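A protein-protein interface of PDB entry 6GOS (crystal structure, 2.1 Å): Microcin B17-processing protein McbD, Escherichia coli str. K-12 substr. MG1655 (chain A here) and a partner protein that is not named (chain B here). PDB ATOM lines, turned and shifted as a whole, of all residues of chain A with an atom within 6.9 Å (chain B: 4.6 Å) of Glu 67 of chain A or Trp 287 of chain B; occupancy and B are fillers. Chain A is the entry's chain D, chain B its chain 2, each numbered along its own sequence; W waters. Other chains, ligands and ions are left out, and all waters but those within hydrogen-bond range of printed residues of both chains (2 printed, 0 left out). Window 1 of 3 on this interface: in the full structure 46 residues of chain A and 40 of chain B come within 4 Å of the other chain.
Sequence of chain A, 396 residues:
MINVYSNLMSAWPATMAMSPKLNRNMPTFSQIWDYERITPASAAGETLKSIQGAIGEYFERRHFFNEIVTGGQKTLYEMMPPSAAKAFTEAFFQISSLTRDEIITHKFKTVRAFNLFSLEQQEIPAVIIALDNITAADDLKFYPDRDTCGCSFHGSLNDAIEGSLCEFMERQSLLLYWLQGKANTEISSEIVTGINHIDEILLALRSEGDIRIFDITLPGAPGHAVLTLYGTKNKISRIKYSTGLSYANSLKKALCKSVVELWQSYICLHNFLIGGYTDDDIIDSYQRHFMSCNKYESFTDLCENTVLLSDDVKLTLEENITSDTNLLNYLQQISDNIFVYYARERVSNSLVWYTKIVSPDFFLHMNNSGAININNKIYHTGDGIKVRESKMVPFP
The backbone carbonyl oxygen (O) of Glu 67 of chain A is in hydrogen-bond range of the indole nitrogen (NE1) of Trp 287 of chain B (3.5 Å).
NH2 of Arg 199 of chain B sits close to NH2 of Arg 62 of chain A, at 3.4 Å.
N of His 286 of chain B sits at hydrogen-bond distance from O of Arg 346 of chain A, at 3.2 Å.
The backbone NH of Gln 288 of chain B is in hydrogen-bond range of the side-chain carboxylate of Glu 345 of chain A (2.8 Å).
OG of Ser 202 of chain B is in hydrogen-bond range of O of Asn 66 of chain A, 2.7 Å away.
The guanidinium group (NH2) of Arg 199 of chain B lies within salt-bridge range of the side-chain carboxylate (OE1) of Glu 345 of chain A (2.8 Å).
The side-chain amide oxygen (OE1) of Gln 288 of chain B sits at hydrogen-bond distance from the guanidinium group (NH1) of Arg 344 of chain A (2.9 Å).
The guanidinium group (NE) of Arg 199 of chain B lies within salt-bridge range of the side-chain carboxylate (OE2) of Glu 67 of chain A (2.8 Å).
The side-chain hydroxyl (OH) of Tyr 58 of chain A sits close to the guanidinium group (NH1) of Arg 62 of chain A, 3.5 Å away.
The side-chain sulfur (SG) of Cys 195 of chain B lies close to the backbone NH (N) of Trp 287 of chain B.
SG of Cys 195 of chain B sits close to ND1 of His 286 of chain B (3.6 Å).
The guanidinium group (NH1) of Arg 199 of chain B is in hydrogen-bond range of the backbone carbonyl oxygen (O) of His 286 of chain B.
OE1 of Glu 345 of chain A lies within hydrogen-bond range of OH of Tyr 354 of chain A, 2.5 Å away.
Among the printed residues, pairs that only touch across the chains: Phe 59 of chain A with Ile 285 of chain B, Glu 67 of chain A with Ser 202 of chain B, Val 69 of chain A with Ala 289 of chain B, Glu 345 of chain A with His 286 of chain B, Glu 345 of chain A with Trp 287 of chain B, Arg 346 of chain A with Ile 285 of chain B and Tyr 354 of chain A with Arg 199 of chain B.
Phe 64 of chain A touches none of the printed residues of chain B.
Of chain B, only Arg 199, Ser 202 and Trp 287 come within 4 Å of Glu 67 of chain A.
Printed residues of chain B within 4 Å of Arg 344 of chain A: Gln 288.
Trp 287 of chain B touches just these residues of chain A: Glu 67 and Glu 345.
Of the printed residues of chain A, Gln 288 of chain B touches Arg 344 and Glu 345.
Of the printed residues of chain A, Ala 289 of chain B touches Val 69.
The nearest residue of chain B that does not touch Glu 67 of chain A is Ala 289 of chain B (4.3 Å).
Of the 19 printed residues of chain A, 9 touch a printed residue of chain B.
Printed residues of chain A that touch a printed residue of chain B: Phe 59, Arg 62, Asn 66, Glu 67, Val 69, Arg 344, Glu 345, Arg 346 and Tyr 354.
Of the 12 printed residues of chain B, 7 touch a printed residue of chain A.
Printed residues of chain B that touch a printed residue of chain A: Arg 199, Ser 202, Ile 285, His 286, Trp 287, Gln 288 and Ala 289.
Hydrophobic or aromatic side chains of chain B that line the printed part of chain A: Ile 285, His 286, Trp 287 and Ala 289.
Along chain B the printed residues that touch a printed residue of chain A span positions 199 to 289.
Among the printed residues, 15 pairs touch across the chains.
Water W1 lies within hydrogen-bond range of the side-chain carboxylate of Glu 345 of chain A (2.6 Å), the side-chain carboxylate of Glu 67 of chain A (2.8 Å), a ring nitrogen (ND1) of His 63 of chain A (3.0 Å) and the guanidinium group of Arg 199 of chain B (3.5 Å).
Water W2 lies within hydrogen-bond range of O of Glu 67 of chain A (2.7 Å) and NE1 of Trp 287 of chain B (3.4 Å).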
ATOM      1  N   ALA A  11     -31.030   3.031  14.111  1.00  0.00           N
ATOM      2  CA  ALA A  11     -29.747   3.735  14.233  1.00  0.00           C
ATOM      3  C   ALA A  11     -29.689   4.969  13.349  1.00  0.00           C
ATOM      4  O   ALA A  11     -28.990   5.924  13.674  1.00  0.00           O
ATOM      5  CB  ALA A  11     -28.591   2.819  13.865  1.00  0.00           C
ATOM      6  N   TYR A  58     -24.164  15.263   8.874  1.00  0.00           N
ATOM      7  CA  TYR A  58     -24.929  14.510   9.862  1.00  0.00           C
ATOM      8  C   TYR A  58     -24.020  13.629  10.720  1.00  0.00           C
ATOM      9  O   TYR A  58     -24.116  13.664  11.940  1.00  0.00           O
ATOM     10  CB  TYR A  58     -26.022  13.630   9.217  1.00  0.00           C
ATOM     11  CG  TYR A  58     -26.674  12.690  10.208  1.00  0.00           C
ATOM     12  CD1 TYR A  58     -27.609  13.171  11.107  1.00  0.00           C
ATOM     13  CD2 TYR A  58     -26.344  11.341  10.264  1.00  0.00           C
ATOM     14  CE1 TYR A  58     -28.192  12.344  12.051  1.00  0.00           C
ATOM     15  CE2 TYR A  58     -26.951  10.484  11.193  1.00  0.00           C
ATOM     16  CZ  TYR A  58     -27.859  11.003  12.094  1.00  0.00           C
ATOM     17  OH  TYR A  58     -28.487  10.230  13.021  1.00  0.00           O
ATOM     18  N   PHE A  59     -23.175  12.821  10.093  1.00  0.00           N
ATOM     19  CA  PHE A  59     -22.237  11.991  10.857  1.00  0.00           C
ATOM     20  C   PHE A  59     -21.374  12.861  11.799  1.00  0.00           C
ATOM     21  O   PHE A  59     -21.218  12.558  12.978  1.00  0.00           O
ATOM     22  CB  PHE A  59     -21.325  11.198   9.939  1.00  0.00           C
ATOM     23  CG  PHE A  59     -21.813   9.810   9.618  1.00  0.00           C
ATOM     24  CD1 PHE A  59     -21.504   8.742  10.459  1.00  0.00           C
ATOM     25  CD2 PHE A  59     -22.534   9.547   8.438  1.00  0.00           C
ATOM     26  CE1 PHE A  59     -21.928   7.445  10.151  1.00  0.00           C
ATOM     27  CE2 PHE A  59     -22.951   8.243   8.113  1.00  0.00           C
ATOM     28  CZ  PHE A  59     -22.643   7.196   8.967  1.00  0.00           C
ATOM     29  N   ARG A  61     -21.860  15.977  13.094  1.00  0.00           N
ATOM     30  CA  ARG A  61     -22.567  16.591  14.196  1.00  0.00           C
ATOM     31  C   ARG A  61     -23.085  15.583  15.218  1.00  0.00           C
ATOM     32  O   ARG A  61     -23.037  15.838  16.435  1.00  0.00           O
ATOM     33  CB  ARG A  61     -23.702  17.456  13.667  1.00  0.00           C
ATOM     34  CG  ARG A  61     -23.165  18.666  12.924  1.00  0.00           C
ATOM     35  CD  ARG A  61     -23.737  19.925  13.518  1.00  0.00           C
ATOM     36  NE  ARG A  61     -25.153  19.987  13.211  1.00  0.00           N
ATOM     37  CZ  ARG A  61     -25.646  20.421  12.060  1.00  0.00           C
ATOM     38  NH1 ARG A  61     -24.860  20.832  11.076  1.00  0.00           N
ATOM     39  NH2 ARG A  61     -26.944  20.440  11.888  1.00  0.00           N
ATOM     40  N   ARG A  62     -23.571  14.442  14.721  1.00  0.00           N
ATOM     41  CA  ARG A  62     -24.029  13.388  15.590  1.00  0.00           C
ATOM     42  C   ARG A  62     -22.875  12.952  16.504  1.00  0.00           C
ATOM     43  O   ARG A  62     -23.071  12.789  17.699  1.00  0.00           O
ATOM     44  CB  ARG A  62     -24.601  12.199  14.812  1.00  0.00           C
ATOM     45  CG  ARG A  62     -25.303  11.188  15.725  1.00  0.00           C
ATOM     46  CD  ARG A  62     -25.899   9.992  14.984  1.00  0.00           C
ATOM     47  NE  ARG A  62     -24.930   9.226  14.195  1.00  0.00           N
ATOM     48  CZ  ARG A  62     -25.195   8.059  13.596  1.00  0.00           C
ATOM     49  NH1 ARG A  62     -26.400   7.493  13.653  1.00  0.00           N
ATOM     50  NH2 ARG A  62     -24.246   7.446  12.917  1.00  0.00           N
ATOM     51  N   HIS A  63     -21.686  12.792  15.937  1.00  0.00           N
ATOM     52  CA  HIS A  63     -20.557  12.313  16.710  1.00  0.00           C
ATOM     53  C   HIS A  63     -20.193  13.281  17.858  1.00  0.00           C
ATOM     54  O   HIS A  63     -20.175  12.887  19.032  1.00  0.00           O
ATOM     55  CB  HIS A  63     -19.354  12.061  15.802  1.00  0.00           C
ATOM     56  CG  HIS A  63     -18.109  11.711  16.547  1.00  0.00           C
ATOM     57  ND1 HIS A  63     -17.850  10.436  17.001  1.00  0.00           N
ATOM     58  CD2 HIS A  63     -17.063  12.476  16.944  1.00  0.00           C
ATOM     59  CE1 HIS A  63     -16.684  10.426  17.625  1.00  0.00           C
ATOM     60  NE2 HIS A  63     -16.185  11.652  17.605  1.00  0.00           N
ATOM     61  N   PHE A  64     -19.942  14.542  17.511  1.00  0.00           N
ATOM     62  CA  PHE A  64     -19.494  15.538  18.498  1.00  0.00           C
ATOM     63  C   PHE A  64     -20.606  15.943  19.478  1.00  0.00           C
ATOM     64  O   PHE A  64     -20.319  16.138  20.655  1.00  0.00           O
ATOM     65  CB  PHE A  64     -18.845  16.758  17.818  1.00  0.00           C
ATOM     66  CG  PHE A  64     -17.538  16.439  17.142  1.00  0.00           C
ATOM     67  CD1 PHE A  64     -16.360  16.336  17.888  1.00  0.00           C
ATOM     68  CD2 PHE A  64     -17.463  16.252  15.760  1.00  0.00           C
ATOM     69  CE1 PHE A  64     -15.151  16.028  17.273  1.00  0.00           C
ATOM     70  CE2 PHE A  64     -16.254  15.947  15.147  1.00  0.00           C
ATOM     71  CZ  PHE A  64     -15.096  15.842  15.906  1.00  0.00           C
ATOM     72  N   PHE A  65     -21.863  16.005  19.020  1.00  0.00           N
ATOM     73  CA  PHE A  65     -22.994  16.361  19.913  1.00  0.00           C
ATOM     74  C   PHE A  65     -23.540  15.194  20.746  1.00  0.00           C
ATOM     75  O   PHE A  65     -23.981  15.425  21.878  1.00  0.00           O
ATOM     76  CB  PHE A  65     -24.179  16.998  19.157  1.00  0.00           C
ATOM     77  CG  PHE A  65     -23.994  18.447  18.790  1.00  0.00           C
ATOM     78  CD1 PHE A  65     -23.320  18.818  17.623  1.00  0.00           C
ATOM     79  CD2 PHE A  65     -24.547  19.446  19.589  1.00  0.00           C
ATOM     80  CE1 PHE A  65     -23.163  20.156  17.285  1.00  0.00           C
ATOM     81  CE2 PHE A  65     -24.396  20.783  19.264  1.00  0.00           C
ATOM     82  CZ  PHE A  65     -23.702  21.140  18.113  1.00  0.00           C
ATOM     83  N   ASN A  66     -23.537  13.964  20.213  1.00  0.00           N
ATOM     84  CA  ASN A  66     -24.329  12.868  20.825  1.00  0.00           C
ATOM     85  C   ASN A  66     -23.572  11.619  21.234  1.00  0.00           C
ATOM     86  O   ASN A  66     -24.172  10.774  21.934  1.00  0.00           O
ATOM     87  CB  ASN A  66     -25.419  12.355  19.875  1.00  0.00           C
ATOM     88  CG  ASN A  66     -26.377  13.415  19.403  1.00  0.00           C
ATOM     89  OD1 ASN A  66     -26.914  13.289  18.294  1.00  0.00           O
ATOM     90  ND2 ASN A  66     -26.633  14.441  20.229  1.00  0.00           N
ATOM     91  N   GLU A  67     -22.314  11.454  20.796  1.00  0.00           N
ATOM     92  CA  GLU A  67     -21.688  10.122  20.800  1.00  0.00           C
ATOM     93  C   GLU A  67     -20.295   9.942  21.436  1.00  0.00           C
ATOM     94  O   GLU A  67     -19.783   8.816  21.414  1.00  0.00           O
ATOM     95  CB  GLU A  67     -21.652   9.602  19.371  1.00  0.00           C
ATOM     96  CG  GLU A  67     -23.034   9.490  18.721  1.00  0.00           C
ATOM     97  CD  GLU A  67     -22.998   8.827  17.356  1.00  0.00           C
ATOM     98  OE1 GLU A  67     -21.920   8.892  16.710  1.00  0.00           O
ATOM     99  OE2 GLU A  67     -24.041   8.244  16.927  1.00  0.00           O
ATOM    100  N   ILE A  68     -19.699  10.995  22.012  1.00  0.00           N
ATOM    101  CA  ILE A  68     -18.340  10.873  22.543  1.00  0.00           C
ATOM    102  C   ILE A  68     -18.408  10.188  23.902  1.00  0.00           C
ATOM    103  O   ILE A  68     -19.217  10.559  24.760  1.00  0.00           O
ATOM    104  CB  ILE A  68     -17.617  12.227  22.767  1.00  0.00           C
ATOM    105  CG1 ILE A  68     -17.721  13.171  21.548  1.00  0.00           C
ATOM    106  CG2 ILE A  68     -16.158  11.995  23.164  1.00  0.00           C
ATOM    107  CD1 ILE A  68     -16.685  12.985  20.471  1.00  0.00           C
ATOM    108  N   VAL A  69     -17.569   9.185  24.094  1.00  0.00           N
ATOM    109  CA  VAL A  69     -17.301   8.671  25.440  1.00  0.00           C
ATOM    110  C   VAL A  69     -15.810   8.902  25.681  1.00  0.00           C
ATOM    111  O   VAL A  69     -14.977   8.524  24.856  1.00  0.00           O
ATOM    112  CB  VAL A  69     -17.707   7.190  25.600  1.00  0.00           C
ATOM    113  CG1 VAL A  69     -17.430   6.694  27.021  1.00  0.00           C
ATOM    114  CG2 VAL A  69     -19.194   7.011  25.270  1.00  0.00           C
ATOM    115  N   ASP A 132     -22.215  18.057  23.966  1.00  0.00           N
ATOM    116  CA  ASP A 132     -23.187  17.804  25.032  1.00  0.00           C
ATOM    117  C   ASP A 132     -22.640  18.200  26.429  1.00  0.00           C
ATOM    118  O   ASP A 132     -21.433  18.378  26.603  1.00  0.00           O
ATOM    119  CB  ASP A 132     -23.558  16.332  25.031  1.00  0.00           C
ATOM    120  CG  ASP A 132     -22.443  15.450  25.563  1.00  0.00           C
ATOM    121  OD1 ASP A 132     -21.466  15.186  24.817  1.00  0.00           O
ATOM    122  OD2 ASP A 132     -22.552  15.045  26.743  1.00  0.00           O
ATOM    123  N   THR A 135     -20.834  14.446  28.872  1.00  0.00           N
ATOM    124  CA  THR A 135     -19.550  13.780  28.628  1.00  0.00           C
ATOM    125  C   THR A 135     -18.435  14.259  29.557  1.00  0.00           C
ATOM    126  O   THR A 135     -17.732  13.441  30.147  1.00  0.00           O
ATOM    127  CB  THR A 135     -19.112  13.987  27.179  1.00  0.00           C
ATOM    128  OG1 THR A 135     -20.114  13.459  26.305  1.00  0.00           O
ATOM    129  CG2 THR A 135     -17.802  13.265  26.896  1.00  0.00           C
ATOM    130  N   TYR A 341      -7.643  15.670  17.283  1.00  0.00           N
ATOM    131  CA  TYR A 341      -8.537  14.676  17.870  1.00  0.00           C
ATOM    132  C   TYR A 341      -9.001  13.809  16.721  1.00  0.00           C
ATOM    133  O   TYR A 341      -9.207  14.293  15.611  1.00  0.00           O
ATOM    134  CB  TYR A 341      -9.758  15.298  18.544  1.00  0.00           C
ATOM    135  CG  TYR A 341     -10.901  14.316  18.719  1.00  0.00           C
ATOM    136  CD1 TYR A 341     -10.899  13.392  19.749  1.00  0.00           C
ATOM    137  CD2 TYR A 341     -11.963  14.297  17.826  1.00  0.00           C
ATOM    138  CE1 TYR A 341     -11.940  12.500  19.918  1.00  0.00           C
ATOM    139  CE2 TYR A 341     -13.007  13.382  17.952  1.00  0.00           C
ATOM    140  CZ  TYR A 341     -12.997  12.483  18.989  1.00  0.00           C
ATOM    141  OH  TYR A 341     -14.020  11.584  19.105  1.00  0.00           O
ATOM    142  N   ARG A 344     -12.778   6.806  14.858  1.00  0.00           N
ATOM    143  CA  ARG A 344     -13.075   6.055  13.671  1.00  0.00           C
ATOM    144  C   ARG A 344     -13.950   4.834  13.965  1.00  0.00           C
ATOM    145  O   ARG A 344     -13.943   4.276  15.084  1.00  0.00           O
ATOM    146  CB  ARG A 344     -11.797   5.707  12.880  1.00  0.00           C
ATOM    147  CG  ARG A 344     -10.907   4.602  13.437  1.00  0.00           C
ATOM    148  CD  ARG A 344     -10.528   4.823  14.885  1.00  0.00           C
ATOM    149  NE  ARG A 344      -9.445   3.946  15.285  1.00  0.00           N
ATOM    150  CZ  ARG A 344      -8.899   3.928  16.501  1.00  0.00           C
ATOM    151  NH1 ARG A 344      -9.354   4.723  17.457  1.00  0.00           N
ATOM    152  NH2 ARG A 344      -7.879   3.114  16.763  1.00  0.00           N
ATOM    153  N   GLU A 345     -14.712   4.475  12.929  1.00  0.00           N
ATOM    154  CA  GLU A 345     -15.741   3.453  12.979  1.00  0.00           C
ATOM    155  C   GLU A 345     -15.752   2.688  11.673  1.00  0.00           C
ATOM    156  O   GLU A 345     -15.747   3.293  10.605  1.00  0.00           O
ATOM    157  CB  GLU A 345     -17.115   4.091  13.208  1.00  0.00           C
ATOM    158  CG  GLU A 345     -17.210   4.657  14.620  1.00  0.00           C
ATOM    159  CD  GLU A 345     -18.466   5.424  14.930  1.00  0.00           C
ATOM    160  OE1 GLU A 345     -19.207   5.828  14.006  1.00  0.00           O
ATOM    161  OE2 GLU A 345     -18.683   5.621  16.142  1.00  0.00           O
ATOM    162  N   ARG A 346     -15.766   1.367  11.770  1.00  0.00           N
ATOM    163  CA  ARG A 346     -15.889   0.519  10.606  1.00  0.00           C
ATOM    164  C   ARG A 346     -17.296   0.589   9.983  1.00  0.00           C
ATOM    165  O   ARG A 346     -18.307   0.525  10.692  1.00  0.00           O
ATOM    166  CB  ARG A 346     -15.533  -0.907  10.957  1.00  0.00           C
ATOM    167  CG  ARG A 346     -15.429  -1.831   9.765  1.00  0.00           C
ATOM    168  CD  ARG A 346     -14.973  -3.213  10.191  1.00  0.00           C
ATOM    169  NE  ARG A 346     -14.851  -4.092   9.037  1.00  0.00           N
ATOM    170  CZ  ARG A 346     -14.456  -5.369   9.089  1.00  0.00           C
ATOM    171  NH1 ARG A 346     -14.158  -5.954  10.248  1.00  0.00           N
ATOM    172  NH2 ARG A 346     -14.359  -6.068   7.958  1.00  0.00           N
ATOM    173  N   TYR A 354     -13.694  10.799  12.078  1.00  0.00           N
ATOM    174  CA  TYR A 354     -14.122  12.051  12.683  1.00  0.00           C
ATOM    175  C   TYR A 354     -12.842  12.705  13.184  1.00  0.00           C
ATOM    176  O   TYR A 354     -12.015  12.023  13.800  1.00  0.00           O
ATOM    177  CB  TYR A 354     -15.066  11.791  13.874  1.00  0.00           C
ATOM    178  CG  TYR A 354     -16.185  10.807  13.596  1.00  0.00           C
ATOM    179  CD1 TYR A 354     -15.979   9.430  13.721  1.00  0.00           C
ATOM    180  CD2 TYR A 354     -17.452  11.247  13.218  1.00  0.00           C
ATOM    181  CE1 TYR A 354     -17.003   8.524  13.459  1.00  0.00           C
ATOM    182  CE2 TYR A 354     -18.490  10.345  12.957  1.00  0.00           C
ATOM    183  CZ  TYR A 354     -18.267   8.987  13.079  1.00  0.00           C
ATOM    184  OH  TYR A 354     -19.292   8.090  12.833  1.00  0.00           O
ATOM    185  N   PHE B 194     -24.445  -3.996  21.309  1.00  0.00           N
ATOM    186  CA  PHE B 194     -24.363  -2.702  21.996  1.00  0.00           C
ATOM    187  C   PHE B 194     -23.906  -1.571  21.092  1.00  0.00           C
ATOM    188  O   PHE B 194     -24.276  -0.442  21.316  1.00  0.00           O
ATOM    189  CB  PHE B 194     -23.494  -2.805  23.257  1.00  0.00           C
ATOM    190  CG  PHE B 194     -24.007  -3.822  24.238  1.00  0.00           C
ATOM    191  CD1 PHE B 194     -25.020  -3.499  25.121  1.00  0.00           C
ATOM    192  CD2 PHE B 194     -23.521  -5.125  24.230  1.00  0.00           C
ATOM    193  CE1 PHE B 194     -25.517  -4.444  26.003  1.00  0.00           C
ATOM    194  CE2 PHE B 194     -24.008  -6.077  25.106  1.00  0.00           C
ATOM    195  CZ  PHE B 194     -25.012  -5.737  25.998  1.00  0.00           C
ATOM    196  N   CYS B 195     -23.112  -1.875  20.071  1.00  0.00           N
ATOM    197  CA  CYS B 195     -22.812  -0.912  19.001  1.00  0.00           C
ATOM    198  C   CYS B 195     -24.068  -0.254  18.451  1.00  0.00           C
ATOM    199  O   CYS B 195     -24.008   0.892  18.030  1.00  0.00           O
ATOM    200  CB  CYS B 195     -22.102  -1.588  17.829  1.00  0.00           C
ATOM    201  SG  CYS B 195     -20.347  -1.917  18.055  1.00  0.00           S
ATOM    202  N   GLU B 198     -26.623   0.725  22.739  1.00  0.00           N
ATOM    203  CA  GLU B 198     -25.978   1.719  23.639  1.00  0.00           C
ATOM    204  C   GLU B 198     -25.757   3.042  22.909  1.00  0.00           C
ATOM    205  O   GLU B 198     -25.960   4.112  23.481  1.00  0.00           O
ATOM    206  CB  GLU B 198     -24.618   1.266  24.224  1.00  0.00           C
ATOM    207  CG  GLU B 198     -24.645   0.255  25.371  1.00  0.00           C
ATOM    208  CD  GLU B 198     -25.593   0.623  26.514  1.00  0.00           C
ATOM    209  OE1 GLU B 198     -25.480   1.752  27.059  1.00  0.00           O
ATOM    210  OE2 GLU B 198     -26.471  -0.223  26.849  1.00  0.00           O
ATOM    211  N   ARG B 199     -25.333   2.953  21.653  1.00  0.00           N
ATOM    212  CA  ARG B 199     -25.217   4.139  20.795  1.00  0.00           C
ATOM    213  C   ARG B 199     -26.552   4.861  20.612  1.00  0.00           C
ATOM    214  O   ARG B 199     -26.600   6.077  20.687  1.00  0.00           O
ATOM    215  CB  ARG B 199     -24.627   3.762  19.437  1.00  0.00           C
ATOM    216  CG  ARG B 199     -24.282   4.944  18.550  1.00  0.00           C
ATOM    217  CD  ARG B 199     -23.673   4.481  17.237  1.00  0.00           C
ATOM    218  NE  ARG B 199     -23.099   5.604  16.496  1.00  0.00           N
ATOM    219  CZ  ARG B 199     -22.153   5.501  15.580  1.00  0.00           C
ATOM    220  NH1 ARG B 199     -21.638   4.322  15.236  1.00  0.00           N
ATOM    221  NH2 ARG B 199     -21.720   6.595  14.998  1.00  0.00           N
ATOM    222  N   SER B 202     -27.274   6.507  23.880  1.00  0.00           N
ATOM    223  CA  SER B 202     -26.382   7.664  23.985  1.00  0.00           C
ATOM    224  C   SER B 202     -26.977   8.879  23.276  1.00  0.00           C
ATOM    225  O   SER B 202     -27.023   9.995  23.840  1.00  0.00           O
ATOM    226  CB  SER B 202     -25.000   7.331  23.414  1.00  0.00           C
ATOM    227  OG  SER B 202     -24.164   8.477  23.365  1.00  0.00           O
ATOM    228  N   ILE B 285     -22.984  -0.474  11.804  1.00  0.00           N
ATOM    229  CA  ILE B 285     -21.628   0.015  11.897  1.00  0.00           C
ATOM    230  C   ILE B 285     -21.109  -0.049  13.353  1.00  0.00           C
ATOM    231  O   ILE B 285     -21.865  -0.213  14.308  1.00  0.00           O
ATOM    232  CB  ILE B 285     -21.513   1.439  11.328  1.00  0.00           C
ATOM    233  CG1 ILE B 285     -22.177   2.482  12.243  1.00  0.00           C
ATOM    234  CG2 ILE B 285     -22.153   1.494   9.934  1.00  0.00           C
ATOM    235  CD1 ILE B 285     -21.995   3.891  11.755  1.00  0.00           C
ATOM    236  N   HIS B 286     -19.799   0.055  13.481  1.00  0.00           N
ATOM    237  CA  HIS B 286     -19.150   0.050  14.769  1.00  0.00           C
ATOM    238  C   HIS B 286     -19.428   1.390  15.442  1.00  0.00           C
ATOM    239  O   HIS B 286     -19.626   2.415  14.763  1.00  0.00           O
ATOM    240  CB  HIS B 286     -17.657  -0.139  14.591  1.00  0.00           C
ATOM    241  CG  HIS B 286     -17.185  -1.539  14.788  1.00  0.00           C
ATOM    242  ND1 HIS B 286     -17.395  -2.225  15.961  1.00  0.00           N
ATOM    243  CD2 HIS B 286     -16.428  -2.346  14.013  1.00  0.00           C
ATOM    244  CE1 HIS B 286     -16.828  -3.410  15.876  1.00  0.00           C
ATOM    245  NE2 HIS B 286     -16.242  -3.513  14.700  1.00  0.00           N
ATOM    246  N   TRP B 287     -19.492   1.362  16.765  1.00  0.00           N
ATOM    247  CA  TRP B 287     -19.542   2.573  17.573  1.00  0.00           C
ATOM    248  C   TRP B 287     -18.156   2.705  18.208  1.00  0.00           C
ATOM    249  O   TRP B 287     -17.743   1.808  18.952  1.00  0.00           O
ATOM    250  CB  TRP B 287     -20.628   2.454  18.635  1.00  0.00           C
ATOM    251  CG  TRP B 287     -20.822   3.665  19.459  1.00  0.00           C
ATOM    252  CD1 TRP B 287     -20.662   4.957  19.073  1.00  0.00           C
ATOM    253  CD2 TRP B 287     -21.246   3.699  20.820  1.00  0.00           C
ATOM    254  NE1 TRP B 287     -20.948   5.808  20.118  1.00  0.00           N
ATOM    255  CE2 TRP B 287     -21.322   5.066  21.202  1.00  0.00           C
ATOM    256  CE3 TRP B 287     -21.577   2.714  21.756  1.00  0.00           C
ATOM    257  CZ2 TRP B 287     -21.710   5.477  22.485  1.00  0.00           C
ATOM    258  CZ3 TRP B 287     -21.967   3.121  23.045  1.00  0.00           C
ATOM    259  CH2 TRP B 287     -22.023   4.500  23.395  1.00  0.00           C
ATOM    260  N   GLN B 288     -17.444   3.805  17.921  1.00  0.00           N
ATOM    261  CA  GLN B 288     -16.084   4.013  18.458  1.00  0.00           C
ATOM    262  C   GLN B 288     -16.040   3.821  20.003  1.00  0.00           C
ATOM    263  O   GLN B 288     -15.051   3.330  20.538  1.00  0.00           O
ATOM    264  CB  GLN B 288     -15.525   5.397  18.041  1.00  0.00           C
ATOM    265  CG  GLN B 288     -14.241   5.861  18.765  1.00  0.00           C
ATOM    266  CD  GLN B 288     -12.970   5.108  18.345  1.00  0.00           C
ATOM    267  OE1 GLN B 288     -12.103   5.662  17.654  1.00  0.00           O
ATOM    268  NE2 GLN B 288     -12.844   3.867  18.776  1.00  0.00           N
ATOM    269  N   ALA B 289     -17.125   4.165  20.695  1.00  0.00           N
ATOM    270  CA  ALA B 289     -17.156   4.083  22.161  1.00  0.00           C
ATOM    271  C   ALA B 289     -17.447   2.693  22.718  1.00  0.00           C
ATOM    272  O   ALA B 289     -17.396   2.508  23.908  1.00  0.00           O
ATOM    273  CB  ALA B 289     -18.178   5.065  22.705  1.00  0.00           C
ATOM    274  N   CYS B 290     -17.771   1.715  21.881  1.00  0.00           N
ATOM    275  CA  CYS B 290     -18.235   0.443  22.388  1.00  0.00           C
ATOM    276  C   CYS B 290     -17.118  -0.387  23.016  1.00  0.00           C
ATOM    277  O   CYS B 290     -15.973  -0.399  22.547  1.00  0.00           O
ATOM    278  CB  CYS B 290     -18.903  -0.362  21.273  1.00  0.00           C
ATOM    279  SG  CYS B 290     -19.773  -1.783  21.946  1.00  0.00           S
ATOM    280  N   LEU B 293     -14.767  -2.880  21.164  1.00  0.00           N
ATOM    281  CA  LEU B 293     -13.511  -2.421  20.554  1.00  0.00           C
ATOM    282  C   LEU B 293     -12.276  -2.437  21.479  1.00  0.00           C
ATOM    283  O   LEU B 293     -11.167  -2.227  20.996  1.00  0.00           O
ATOM    284  CB  LEU B 293     -13.686  -1.043  19.897  1.00  0.00           C
ATOM    285  CG  LEU B 293     -14.571  -1.027  18.638  1.00  0.00           C
ATOM    286  CD1 LEU B 293     -14.575   0.360  18.021  1.00  0.00           C
ATOM    287  CD2 LEU B 293     -14.125  -2.046  17.611  1.00  0.00           C
HETATM  288  O   HOH W   1     -19.370   7.894  17.167  1.00  0.00           O
HETATM  289  O   HOH W   2     -18.165   7.713  19.510  1.00  0.00           O
